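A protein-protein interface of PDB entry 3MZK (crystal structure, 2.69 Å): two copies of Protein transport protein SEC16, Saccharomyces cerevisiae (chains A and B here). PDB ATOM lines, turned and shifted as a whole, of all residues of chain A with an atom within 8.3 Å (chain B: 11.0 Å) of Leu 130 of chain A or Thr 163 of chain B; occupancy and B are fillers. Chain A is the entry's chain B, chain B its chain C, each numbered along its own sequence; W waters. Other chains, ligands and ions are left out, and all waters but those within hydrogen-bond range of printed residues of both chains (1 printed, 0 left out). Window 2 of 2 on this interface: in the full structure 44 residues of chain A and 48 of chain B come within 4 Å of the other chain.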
ATOM      1  N   LYS A 117      29.768  -0.430   3.517  1.00  0.00           N
ATOM      2  CA  LYS A 117      29.375  -0.695   4.892  1.00  0.00           C
ATOM      3  C   LYS A 117      29.258   0.629   5.636  1.00  0.00           C
ATOM      4  O   LYS A 117      28.242   0.914   6.273  1.00  0.00           O
ATOM      5  CB  LYS A 117      30.395  -1.603   5.582  1.00  0.00           C
ATOM      6  N   SER A 120      26.414   2.717   4.392  1.00  0.00           N
ATOM      7  CA  SER A 120      25.180   2.093   4.844  1.00  0.00           C
ATOM      8  C   SER A 120      24.871   2.473   6.288  1.00  0.00           C
ATOM      9  O   SER A 120      23.749   2.864   6.606  1.00  0.00           O
ATOM     10  CB  SER A 120      25.264   0.571   4.702  1.00  0.00           C
ATOM     11  OG  SER A 120      24.102  -0.059   5.216  1.00  0.00           O
ATOM     12  N   TYR A 124      21.691   4.594   8.117  1.00  0.00           N
ATOM     13  CA  TYR A 124      20.836   3.898   9.071  1.00  0.00           C
ATOM     14  C   TYR A 124      21.654   3.069  10.044  1.00  0.00           C
ATOM     15  O   TYR A 124      22.380   2.160   9.637  1.00  0.00           O
ATOM     16  CB  TYR A 124      19.860   3.001   8.312  1.00  0.00           C
ATOM     17  CG  TYR A 124      18.824   2.317   9.167  1.00  0.00           C
ATOM     18  CD1 TYR A 124      17.713   3.009   9.638  1.00  0.00           C
ATOM     19  CD2 TYR A 124      18.939   0.967   9.479  1.00  0.00           C
ATOM     20  CE1 TYR A 124      16.753   2.377  10.410  1.00  0.00           C
ATOM     21  CE2 TYR A 124      17.985   0.324  10.250  1.00  0.00           C
ATOM     22  CZ  TYR A 124      16.897   1.032  10.712  1.00  0.00           C
ATOM     23  OH  TYR A 124      15.951   0.391  11.478  1.00  0.00           O
ATOM     24  N   ASN A 125      21.543   3.389  11.329  1.00  0.00           N
ATOM     25  CA  ASN A 125      22.223   2.618  12.359  1.00  0.00           C
ATOM     26  C   ASN A 125      21.577   1.255  12.518  1.00  0.00           C
ATOM     27  O   ASN A 125      20.441   1.150  12.972  1.00  0.00           O
ATOM     28  CB  ASN A 125      22.189   3.345  13.697  1.00  0.00           C
ATOM     29  CG  ASN A 125      22.814   2.529  14.807  1.00  0.00           C
ATOM     30  OD1 ASN A 125      23.774   1.794  14.577  1.00  0.00           O
ATOM     31  ND2 ASN A 125      22.265   2.637  16.015  1.00  0.00           N
ATOM     32  N   SER A 126      22.304   0.210  12.147  1.00  0.00           N
ATOM     33  CA  SER A 126      21.749  -1.138  12.160  1.00  0.00           C
ATOM     34  C   SER A 126      21.928  -1.826  13.509  1.00  0.00           C
ATOM     35  O   SER A 126      21.425  -2.925  13.721  1.00  0.00           O
ATOM     36  CB  SER A 126      22.367  -1.988  11.045  1.00  0.00           C
ATOM     37  OG  SER A 126      23.761  -2.158  11.235  1.00  0.00           O
ATOM     38  N   ASP A 127      22.639  -1.166  14.417  1.00  0.00           N
ATOM     39  CA  ASP A 127      22.935  -1.736  15.728  1.00  0.00           C
ATOM     40  C   ASP A 127      21.674  -2.033  16.540  1.00  0.00           C
ATOM     41  O   ASP A 127      21.658  -2.943  17.371  1.00  0.00           O
ATOM     42  CB  ASP A 127      23.875  -0.818  16.514  1.00  0.00           C
ATOM     43  CG  ASP A 127      25.204  -0.609  15.811  1.00  0.00           C
ATOM     44  OD1 ASP A 127      25.488  -1.347  14.840  1.00  0.00           O
ATOM     45  OD2 ASP A 127      25.967   0.288  16.232  1.00  0.00           O
ATOM     46  N   GLU A 128      20.621  -1.263  16.291  1.00  0.00           N
ATOM     47  CA  GLU A 128      19.334  -1.497  16.930  1.00  0.00           C
ATOM     48  C   GLU A 128      18.856  -2.914  16.630  1.00  0.00           C
ATOM     49  O   GLU A 128      18.301  -3.594  17.495  1.00  0.00           O
ATOM     50  CB  GLU A 128      18.310  -0.484  16.425  1.00  0.00           C
ATOM     51  CG  GLU A 128      18.793   0.959  16.476  1.00  0.00           C
ATOM     52  CD  GLU A 128      17.898   1.910  15.704  1.00  0.00           C
ATOM     53  OE1 GLU A 128      17.059   1.433  14.909  1.00  0.00           O
ATOM     54  OE2 GLU A 128      18.033   3.137  15.893  1.00  0.00           O
ATOM     55  N   LEU A 129      19.092  -3.353  15.395  1.00  0.00           N
ATOM     56  CA  LEU A 129      18.650  -4.665  14.926  1.00  0.00           C
ATOM     57  C   LEU A 129      19.474  -5.828  15.476  1.00  0.00           C
ATOM     58  O   LEU A 129      18.958  -6.933  15.637  1.00  0.00           O
ATOM     59  CB  LEU A 129      18.668  -4.714  13.399  1.00  0.00           C
ATOM     60  CG  LEU A 129      17.704  -3.797  12.645  1.00  0.00           C
ATOM     61  CD1 LEU A 129      18.120  -3.680  11.189  1.00  0.00           C
ATOM     62  CD2 LEU A 129      16.270  -4.297  12.761  1.00  0.00           C
ATOM     63  N   LEU A 130      20.754  -5.588  15.745  1.00  0.00           N
ATOM     64  CA  LEU A 130      21.627  -6.628  16.284  1.00  0.00           C
ATOM     65  C   LEU A 130      21.118  -7.119  17.631  1.00  0.00           C
ATOM     66  O   LEU A 130      21.253  -8.297  17.967  1.00  0.00           O
ATOM     67  CB  LEU A 130      23.059  -6.115  16.427  1.00  0.00           C
ATOM     68  CG  LEU A 130      23.757  -5.698  15.134  1.00  0.00           C
ATOM     69  CD1 LEU A 130      25.131  -5.111  15.434  1.00  0.00           C
ATOM     70  CD2 LEU A 130      23.858  -6.873  14.172  1.00  0.00           C
ATOM     71  N   MET A 131      20.538  -6.203  18.400  1.00  0.00           N
ATOM     72  CA  MET A 131      19.931  -6.548  19.678  1.00  0.00           C
ATOM     73  C   MET A 131      18.837  -7.578  19.449  1.00  0.00           C
ATOM     74  O   MET A 131      18.809  -8.633  20.080  1.00  0.00           O
ATOM     75  CB  MET A 131      19.330  -5.302  20.330  1.00  0.00           C
ATOM     76  CG  MET A 131      20.329  -4.185  20.593  1.00  0.00           C
ATOM     77  SD  MET A 131      21.577  -4.666  21.797  1.00  0.00           S
ATOM     78  CE  MET A 131      20.538  -5.369  23.076  1.00  0.00           C
ATOM     79  N   TYR A 132      17.940  -7.254  18.527  1.00  0.00           N
ATOM     80  CA  TYR A 132      16.824  -8.120  18.181  1.00  0.00           C
ATOM     81  C   TYR A 132      17.275  -9.512  17.736  1.00  0.00           C
ATOM     82  O   TYR A 132      16.655 -10.514  18.086  1.00  0.00           O
ATOM     83  CB  TYR A 132      15.977  -7.451  17.096  1.00  0.00           C
ATOM     84  CG  TYR A 132      14.999  -8.364  16.400  1.00  0.00           C
ATOM     85  CD1 TYR A 132      15.157  -8.683  15.060  1.00  0.00           C
ATOM     86  CD2 TYR A 132      13.917  -8.906  17.079  1.00  0.00           C
ATOM     87  CE1 TYR A 132      14.265  -9.518  14.413  1.00  0.00           C
ATOM     88  CE2 TYR A 132      13.020  -9.743  16.443  1.00  0.00           C
ATOM     89  CZ  TYR A 132      13.199 -10.045  15.109  1.00  0.00           C
ATOM     90  OH  TYR A 132      12.309 -10.875  14.469  1.00  0.00           O
ATOM     91  N   LEU A 133      18.362  -9.573  16.974  1.00  0.00           N
ATOM     92  CA  LEU A 133      18.835 -10.840  16.426  1.00  0.00           C
ATOM     93  C   LEU A 133      19.525 -11.723  17.463  1.00  0.00           C
ATOM     94  O   LEU A 133      19.618 -12.941  17.289  1.00  0.00           O
ATOM     95  CB  LEU A 133      19.757 -10.601  15.231  1.00  0.00           C
ATOM     96  CG  LEU A 133      19.031 -10.099  13.986  1.00  0.00           C
ATOM     97  CD1 LEU A 133      20.009  -9.851  12.851  1.00  0.00           C
ATOM     98  CD2 LEU A 133      17.960 -11.096  13.569  1.00  0.00           C
ATOM     99  N   SER A 134      20.006 -11.108  18.538  1.00  0.00           N
ATOM    100  CA  SER A 134      20.649 -11.854  19.613  1.00  0.00           C
ATOM    101  C   SER A 134      19.610 -12.564  20.477  1.00  0.00           C
ATOM    102  O   SER A 134      19.879 -13.630  21.027  1.00  0.00           O
ATOM    103  CB  SER A 134      21.537 -10.937  20.466  1.00  0.00           C
ATOM    104  OG  SER A 134      20.782  -9.938  21.128  1.00  0.00           O
ATOM    105  N   GLN A 135      18.425 -11.972  20.588  1.00  0.00           N
ATOM    106  CA  GLN A 135      17.333 -12.575  21.342  1.00  0.00           C
ATOM    107  C   GLN A 135      17.095 -14.002  20.869  1.00  0.00           C
ATOM    108  O   GLN A 135      16.949 -14.246  19.671  1.00  0.00           O
ATOM    109  CB  GLN A 135      16.053 -11.755  21.188  1.00  0.00           C
ATOM    110  N   ILE A 223      14.486  -5.294  -2.229  1.00  0.00           N
ATOM    111  CA  ILE A 223      15.843  -5.830  -2.147  1.00  0.00           C
ATOM    112  C   ILE A 223      16.114  -6.890  -3.210  1.00  0.00           C
ATOM    113  O   ILE A 223      17.166  -6.884  -3.849  1.00  0.00           O
ATOM    114  CB  ILE A 223      16.121  -6.449  -0.768  1.00  0.00           C
ATOM    115  CG1 ILE A 223      16.012  -5.382   0.319  1.00  0.00           C
ATOM    116  CG2 ILE A 223      17.500  -7.066  -0.740  1.00  0.00           C
ATOM    117  CD1 ILE A 223      16.281  -5.899   1.704  1.00  0.00           C
ATOM    118  N   SER A 254      16.662   3.707   5.427  1.00  0.00           N
ATOM    119  CA  SER A 254      16.920   2.306   5.743  1.00  0.00           C
ATOM    120  C   SER A 254      16.867   1.430   4.497  1.00  0.00           C
ATOM    121  O   SER A 254      17.525   0.395   4.430  1.00  0.00           O
ATOM    122  CB  SER A 254      15.930   1.798   6.793  1.00  0.00           C
ATOM    123  OG  SER A 254      14.592   2.017   6.381  1.00  0.00           O
ATOM    124  N   ALA A 257      20.130   1.895   2.659  1.00  0.00           N
ATOM    125  CA  ALA A 257      21.129   1.283   3.534  1.00  0.00           C
ATOM    126  C   ALA A 257      21.132  -0.237   3.403  1.00  0.00           C
ATOM    127  O   ALA A 257      22.189  -0.865   3.426  1.00  0.00           O
ATOM    128  CB  ALA A 257      20.903   1.698   4.985  1.00  0.00           C
ATOM    129  N   ALA A 258      19.946  -0.818   3.261  1.00  0.00           N
ATOM    130  CA  ALA A 258      19.817  -2.257   3.077  1.00  0.00           C
ATOM    131  C   ALA A 258      20.481  -2.696   1.780  1.00  0.00           C
ATOM    132  O   ALA A 258      21.208  -3.691   1.749  1.00  0.00           O
ATOM    133  CB  ALA A 258      18.357  -2.672   3.091  1.00  0.00           C
ATOM    134  N   ILE A 261      24.490  -2.350   1.926  1.00  0.00           N
ATOM    135  CA  ILE A 261      25.156  -3.287   2.824  1.00  0.00           C
ATOM    136  C   ILE A 261      25.139  -4.704   2.264  1.00  0.00           C
ATOM    137  O   ILE A 261      25.845  -5.577   2.756  1.00  0.00           O
ATOM    138  CB  ILE A 261      24.527  -3.273   4.232  1.00  0.00           C
ATOM    139  CG1 ILE A 261      25.553  -3.696   5.283  1.00  0.00           C
ATOM    140  CG2 ILE A 261      23.287  -4.147   4.275  1.00  0.00           C
ATOM    141  CD1 ILE A 261      25.070  -3.511   6.712  1.00  0.00           C
ATOM    142  N   ASN A 262      24.335  -4.926   1.230  1.00  0.00           N
ATOM    143  CA  ASN A 262      24.246  -6.236   0.598  1.00  0.00           C
ATOM    144  C   ASN A 262      25.034  -6.317  -0.699  1.00  0.00           C
ATOM    145  O   ASN A 262      24.917  -7.288  -1.445  1.00  0.00           O
ATOM    146  CB  ASN A 262      22.789  -6.611   0.337  1.00  0.00           C
ATOM    147  CG  ASN A 262      22.075  -7.052   1.587  1.00  0.00           C
ATOM    148  OD1 ASN A 262      22.594  -7.856   2.355  1.00  0.00           O
ATOM    149  ND2 ASN A 262      20.882  -6.521   1.807  1.00  0.00           N
ATOM    150  N   MET B 155      10.636 -11.914   9.717  1.00  0.00           N
ATOM    151  CA  MET B 155      11.258 -10.710  10.266  1.00  0.00           C
ATOM    152  C   MET B 155      12.757 -10.901  10.467  1.00  0.00           C
ATOM    153  O   MET B 155      13.552 -10.014  10.156  1.00  0.00           O
ATOM    154  CB  MET B 155      10.602 -10.297  11.588  1.00  0.00           C
ATOM    155  CG  MET B 155       9.158  -9.853  11.448  1.00  0.00           C
ATOM    156  SD  MET B 155       8.460  -9.245  12.991  1.00  0.00           S
ATOM    157  CE  MET B 155       8.836 -10.601  14.101  1.00  0.00           C
ATOM    158  N   ARG B 156      13.139 -12.061  10.990  1.00  0.00           N
ATOM    159  CA  ARG B 156      14.547 -12.363  11.212  1.00  0.00           C
ATOM    160  C   ARG B 156      15.344 -12.246   9.921  1.00  0.00           C
ATOM    161  O   ARG B 156      16.411 -11.630   9.890  1.00  0.00           O
ATOM    162  CB  ARG B 156      14.717 -13.761  11.814  1.00  0.00           C
ATOM    163  CG  ARG B 156      14.229 -13.875  13.247  1.00  0.00           C
ATOM    164  CD  ARG B 156      14.588 -15.219  13.852  1.00  0.00           C
ATOM    165  NE  ARG B 156      16.031 -15.437  13.929  1.00  0.00           N
ATOM    166  CZ  ARG B 156      16.807 -14.989  14.913  1.00  0.00           C
ATOM    167  NH1 ARG B 156      16.287 -14.285  15.912  1.00  0.00           N
ATOM    168  NH2 ARG B 156      18.109 -15.242  14.895  1.00  0.00           N
ATOM    169  N   VAL B 157      14.814 -12.837   8.856  1.00  0.00           N
ATOM    170  CA  VAL B 157      15.471 -12.806   7.557  1.00  0.00           C
ATOM    171  C   VAL B 157      15.672 -11.379   7.070  1.00  0.00           C
ATOM    172  O   VAL B 157      16.742 -11.028   6.572  1.00  0.00           O
ATOM    173  CB  VAL B 157      14.675 -13.593   6.508  1.00  0.00           C
ATOM    174  CG1 VAL B 157      15.286 -13.405   5.133  1.00  0.00           C
ATOM    175  CG2 VAL B 157      14.639 -15.063   6.878  1.00  0.00           C
ATOM    176  N   LEU B 158      14.641 -10.555   7.221  1.00  0.00           N
ATOM    177  CA  LEU B 158      14.744  -9.159   6.816  1.00  0.00           C
ATOM    178  C   LEU B 158      15.827  -8.455   7.619  1.00  0.00           C
ATOM    179  O   LEU B 158      16.706  -7.808   7.053  1.00  0.00           O
ATOM    180  CB  LEU B 158      13.404  -8.437   6.968  1.00  0.00           C
ATOM    181  CG  LEU B 158      13.426  -6.947   6.610  1.00  0.00           C
ATOM    182  CD1 LEU B 158      14.197  -6.697   5.323  1.00  0.00           C
ATOM    183  CD2 LEU B 158      12.017  -6.409   6.496  1.00  0.00           C
ATOM    184  N   ALA B 159      15.768  -8.595   8.937  1.00  0.00           N
ATOM    185  CA  ALA B 159      16.771  -7.991   9.805  1.00  0.00           C
ATOM    186  C   ALA B 159      18.177  -8.476   9.452  1.00  0.00           C
ATOM    187  O   ALA B 159      19.135  -7.704   9.472  1.00  0.00           O
ATOM    188  CB  ALA B 159      16.455  -8.277  11.263  1.00  0.00           C
ATOM    189  N   PHE B 160      18.294  -9.760   9.128  1.00  0.00           N
ATOM    190  CA  PHE B 160      19.574 -10.322   8.720  1.00  0.00           C
ATOM    191  C   PHE B 160      20.090  -9.612   7.478  1.00  0.00           C
ATOM    192  O   PHE B 160      21.272  -9.282   7.394  1.00  0.00           O
ATOM    193  CB  PHE B 160      19.451 -11.822   8.444  1.00  0.00           C
ATOM    194  CG  PHE B 160      19.731 -12.683   9.635  1.00  0.00           C
ATOM    195  CD1 PHE B 160      20.753 -12.363  10.512  1.00  0.00           C
ATOM    196  CD2 PHE B 160      18.973 -13.816   9.881  1.00  0.00           C
ATOM    197  CE1 PHE B 160      21.016 -13.159  11.612  1.00  0.00           C
ATOM    198  CE2 PHE B 160      19.229 -14.611  10.979  1.00  0.00           C
ATOM    199  CZ  PHE B 160      20.252 -14.280  11.848  1.00  0.00           C
ATOM    200  N   LEU B 161      19.199  -9.389   6.516  1.00  0.00           N
ATOM    201  CA  LEU B 161      19.567  -8.722   5.271  1.00  0.00           C
ATOM    202  C   LEU B 161      19.874  -7.244   5.496  1.00  0.00           C
ATOM    203  O   LEU B 161      20.776  -6.683   4.873  1.00  0.00           O
ATOM    204  CB  LEU B 161      18.462  -8.886   4.232  1.00  0.00           C
ATOM    205  CG  LEU B 161      18.267 -10.318   3.738  1.00  0.00           C
ATOM    206  CD1 LEU B 161      17.102 -10.399   2.772  1.00  0.00           C
ATOM    207  CD2 LEU B 161      19.536 -10.828   3.085  1.00  0.00           C
ATOM    208  N   GLN B 162      19.125  -6.617   6.396  1.00  0.00           N
ATOM    209  CA  GLN B 162      19.358  -5.221   6.733  1.00  0.00           C
ATOM    210  C   GLN B 162      20.717  -5.025   7.393  1.00  0.00           C
ATOM    211  O   GLN B 162      21.224  -3.907   7.468  1.00  0.00           O
ATOM    212  CB  GLN B 162      18.260  -4.704   7.656  1.00  0.00           C
ATOM    213  CG  GLN B 162      16.910  -4.535   6.992  1.00  0.00           C
ATOM    214  CD  GLN B 162      15.942  -3.775   7.873  1.00  0.00           C
ATOM    215  OE1 GLN B 162      15.031  -4.359   8.457  1.00  0.00           O
ATOM    216  NE2 GLN B 162      16.139  -2.463   7.981  1.00  0.00           N
ATOM    217  N   THR B 163      21.305  -6.114   7.872  1.00  0.00           N
ATOM    218  CA  THR B 163      22.616  -6.049   8.515  1.00  0.00           C
ATOM    219  C   THR B 163      23.708  -6.630   7.623  1.00  0.00           C
ATOM    220  O   THR B 163      24.873  -6.701   8.020  1.00  0.00           O
ATOM    221  CB  THR B 163      22.621  -6.774   9.873  1.00  0.00           C
ATOM    222  OG1 THR B 163      22.102  -8.099   9.711  1.00  0.00           O
ATOM    223  CG2 THR B 163      21.761  -6.026  10.878  1.00  0.00           C
ATOM    224  N   GLY B 164      23.319  -7.042   6.417  1.00  0.00           N
ATOM    225  CA  GLY B 164      24.257  -7.547   5.432  1.00  0.00           C
ATOM    226  C   GLY B 164      24.664  -8.997   5.628  1.00  0.00           C
ATOM    227  O   GLY B 164      25.659  -9.450   5.060  1.00  0.00           O
ATOM    228  N   ASN B 165      23.889  -9.729   6.421  1.00  0.00           N
ATOM    229  CA  ASN B 165      24.235 -11.099   6.778  1.00  0.00           C
ATOM    230  C   ASN B 165      23.582 -12.142   5.876  1.00  0.00           C
ATOM    231  O   ASN B 165      22.573 -12.745   6.236  1.00  0.00           O
ATOM    232  CB  ASN B 165      23.863 -11.368   8.234  1.00  0.00           C
ATOM    233  CG  ASN B 165      24.637 -12.528   8.830  1.00  0.00           C
ATOM    234  OD1 ASN B 165      25.188 -13.365   8.112  1.00  0.00           O
ATOM    235  ND2 ASN B 165      24.675 -12.587  10.151  1.00  0.00           N
ATOM    236  N   HIS B 166      24.171 -12.355   4.705  1.00  0.00           N
ATOM    237  CA  HIS B 166      23.642 -13.318   3.750  1.00  0.00           C
ATOM    238  C   HIS B 166      23.682 -14.729   4.313  1.00  0.00           C
ATOM    239  O   HIS B 166      22.702 -15.473   4.239  1.00  0.00           O
ATOM    240  CB  HIS B 166      24.448 -13.277   2.453  1.00  0.00           C
ATOM    241  CG  HIS B 166      24.313 -11.990   1.700  1.00  0.00           C
ATOM    242  ND1 HIS B 166      25.083 -11.698   0.593  1.00  0.00           N
ATOM    243  CD2 HIS B 166      23.499 -10.934   1.888  1.00  0.00           C
ATOM    244  CE1 HIS B 166      24.744 -10.507   0.136  1.00  0.00           C
ATOM    245  NE2 HIS B 166      23.788 -10.018   0.897  1.00  0.00           N
ATOM    246  N   ASP B 167      24.829 -15.095   4.870  1.00  0.00           N
ATOM    247  CA  ASP B 167      25.046 -16.452   5.337  1.00  0.00           C
ATOM    248  C   ASP B 167      24.048 -16.839   6.420  1.00  0.00           C
ATOM    249  O   ASP B 167      23.497 -17.937   6.401  1.00  0.00           O
ATOM    250  CB  ASP B 167      26.479 -16.621   5.843  1.00  0.00           C
ATOM    251  CG  ASP B 167      27.512 -16.358   4.762  1.00  0.00           C
ATOM    252  OD1 ASP B 167      28.460 -17.164   4.638  1.00  0.00           O
ATOM    253  OD2 ASP B 167      27.379 -15.344   4.040  1.00  0.00           O
ATOM    254  N   GLU B 168      23.811 -15.936   7.362  1.00  0.00           N
ATOM    255  CA  GLU B 168      22.905 -16.238   8.456  1.00  0.00           C
ATOM    256  C   GLU B 168      21.466 -16.290   7.960  1.00  0.00           C
ATOM    257  O   GLU B 168      20.654 -17.069   8.459  1.00  0.00           O
ATOM    258  CB  GLU B 168      23.053 -15.221   9.586  1.00  0.00           C
ATOM    259  CG  GLU B 168      22.930 -15.835  10.969  1.00  0.00           C
ATOM    260  CD  GLU B 168      23.942 -16.939  11.208  1.00  0.00           C
ATOM    261  OE1 GLU B 168      25.158 -16.653  11.150  1.00  0.00           O
ATOM    262  OE2 GLU B 168      23.523 -18.093  11.446  1.00  0.00           O
ATOM    263  N   ALA B 169      21.161 -15.458   6.971  1.00  0.00           N
ATOM    264  CA  ALA B 169      19.832 -15.432   6.371  1.00  0.00           C
ATOM    265  C   ALA B 169      19.533 -16.749   5.653  1.00  0.00           C
ATOM    266  O   ALA B 169      18.450 -17.314   5.798  1.00  0.00           O
ATOM    267  CB  ALA B 169      19.702 -14.250   5.416  1.00  0.00           C
ATOM    268  N   LEU B 170      20.501 -17.239   4.887  1.00  0.00           N
ATOM    269  CA  LEU B 170      20.328 -18.485   4.152  1.00  0.00           C
ATOM    270  C   LEU B 170      20.220 -19.685   5.086  1.00  0.00           C
ATOM    271  O   LEU B 170      19.370 -20.560   4.893  1.00  0.00           O
ATOM    272  CB  LEU B 170      21.486 -18.699   3.183  1.00  0.00           C
ATOM    273  CG  LEU B 170      21.429 -19.992   2.369  1.00  0.00           C
ATOM    274  CD1 LEU B 170      20.142 -20.063   1.560  1.00  0.00           C
ATOM    275  CD2 LEU B 170      22.645 -20.115   1.462  1.00  0.00           C
ATOM    276  N   LEU B 172      19.116 -19.812   8.026  1.00  0.00           N
ATOM    277  CA  LEU B 172      17.812 -19.817   8.671  1.00  0.00           C
ATOM    278  C   LEU B 172      16.709 -20.299   7.731  1.00  0.00           C
ATOM    279  O   LEU B 172      15.821 -21.047   8.135  1.00  0.00           O
ATOM    280  CB  LEU B 172      17.475 -18.429   9.223  1.00  0.00           C
ATOM    281  CG  LEU B 172      16.068 -18.312   9.810  1.00  0.00           C
ATOM    282  CD1 LEU B 172      15.848 -19.365  10.884  1.00  0.00           C
ATOM    283  CD2 LEU B 172      15.829 -16.917  10.353  1.00  0.00           C
ATOM    284  N   LEU B 188      21.540 -13.531  -4.148  1.00  0.00           N
ATOM    285  CA  LEU B 188      22.365 -12.398  -3.740  1.00  0.00           C
ATOM    286  C   LEU B 188      23.801 -12.822  -3.443  1.00  0.00           C
ATOM    287  O   LEU B 188      24.647 -11.983  -3.141  1.00  0.00           O
ATOM    288  CB  LEU B 188      21.786 -11.730  -2.495  1.00  0.00           C
ATOM    289  CG  LEU B 188      20.314 -11.322  -2.502  1.00  0.00           C
ATOM    290  CD1 LEU B 188      19.960 -10.615  -1.198  1.00  0.00           C
ATOM    291  CD2 LEU B 188      20.008 -10.433  -3.691  1.00  0.00           C
HETATM  292  O   HOH W   1      22.137  -0.598   7.497  1.00  0.00           O
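The side-chain amide nitrogen of Asn 262 of chain A sits at hydrogen-bond distance from the backbone carbonyl oxygen of Leu 161 of chain B (3.1 Å). A ring nitrogen (NE2) of His 166 of chain B is in hydrogen-bond range of the side-chain amide oxygen (OD1) of Asn 262 of chain A, 2.9 Å away.
O of Ala 258 of chain A is in hydrogen-bond range of ND2 of Asn 262 of chain A (2.8 Å). The side-chain hydroxyl (OG1) of Thr 163 of chain B sits at hydrogen-bond distance from the backbone carbonyl oxygen (O) of Ala 159 of chain B, 3.0 Å away. The backbone carbonyl oxygen (O) of Phe 160 of chain B lies within hydrogen-bond range of the side-chain hydroxyl (OG1) of Thr 163 of chain B (2.7 Å). The backbone NH (N) of Asn 165 of chain B lies within hydrogen-bond range of the backbone carbonyl oxygen (O) of Phe 160 of chain B (2.8 Å).
Among the printed residues, merely in contact across the chains: Tyr 132 of chain A with Met 155 of chain B, Ile 261 of chain A with Thr 163 of chain B, Asn 262 of chain A with Gly 164 of chain B, Leu 133 of chain A with Phe 160 of chain B, Ile 261 of chain A with Gly 164 of chain B, Ile 261 of chain A with Leu 161 of chain B, Leu 133 of chain A with Arg 156 of chain B, Leu 129 of chain A with Gln 162 of chain B, Tyr 132 of chain A with Arg 156 of chain B, Ile 261 of chain A with Gln 162 of chain B, Gln 135 of chain A with Arg 156 of chain B, Leu 133 of chain A with Ala 159 of chain B and Leu 130 of chain A with Thr 163 of chain B.
Of the printed residues of chain B, Leu 130 of chain A touches Thr 163. Printed residues of chain A within 4 Å of Thr 163 of chain B: Leu 130 (3.996 Å) and Ile 261 (3.5 Å). No residue of chain B comes within 4 Å of Ser 126 of chain A. Leu 129 of chain A touches one residue of chain B. Of chain B, only Arg 156 (3.6 Å), Ala 159 (3.9 Å) and Phe 160 (3.5 Å) come within 4 Å of Leu 133 of chain A. No residue of chain B comes within 4 Å of Ser 134 of chain A. Gly 164 of chain B touches just these residues of chain A: Ile 261 and Asn 262. Of the printed residues of chain A, His 166 of chain B touches Asn 262 (2.9 Å). Printed residues of chain B within 4 Å of Tyr 132 of chain A: Met 155 and Arg 156. Printed residues of chain A within 4 Å of Gln 162 of chain B: Leu 129 and Ile 261. Asn 165 of chain B touches none of the printed residues of chain A. Leu 158 of chain B touches none of the printed residues of chain A. The nearest printed residue of chain A that does not touch Thr 163 of chain B is Ser 126 of chain A (4.1 Å). The nearest printed residue of chain A that does not touch His 166 of chain B is Ile 261 of chain A (5.2 Å).
Hydrophobic or aromatic side chains of chain A that line the printed part of chain B: Leu 129, Leu 130, Tyr 132, Leu 133 and Ile 261. Hydrophobic or aromatic side chains of chain B within 4 Å of the printed part of chain A: Met 155, Ala 159, Phe 160 and His 166. Among the printed residues, 15 pairs touch across the chains.
No position is printed for both chains. Of the 15 pairs that touch across the chains among the printed residues, none has its exchanged pair printed and touching as well.
Water W1 lies within hydrogen-bond range of the side-chain hydroxyl (OG) of Ser 120 of chain A (3.1 Å), the backbone carbonyl oxygen (O) of Gln 162 of chain B (3.4 Å) and the backbone carbonyl oxygen (O) of Tyr 124 of chain A (3.5 Å).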
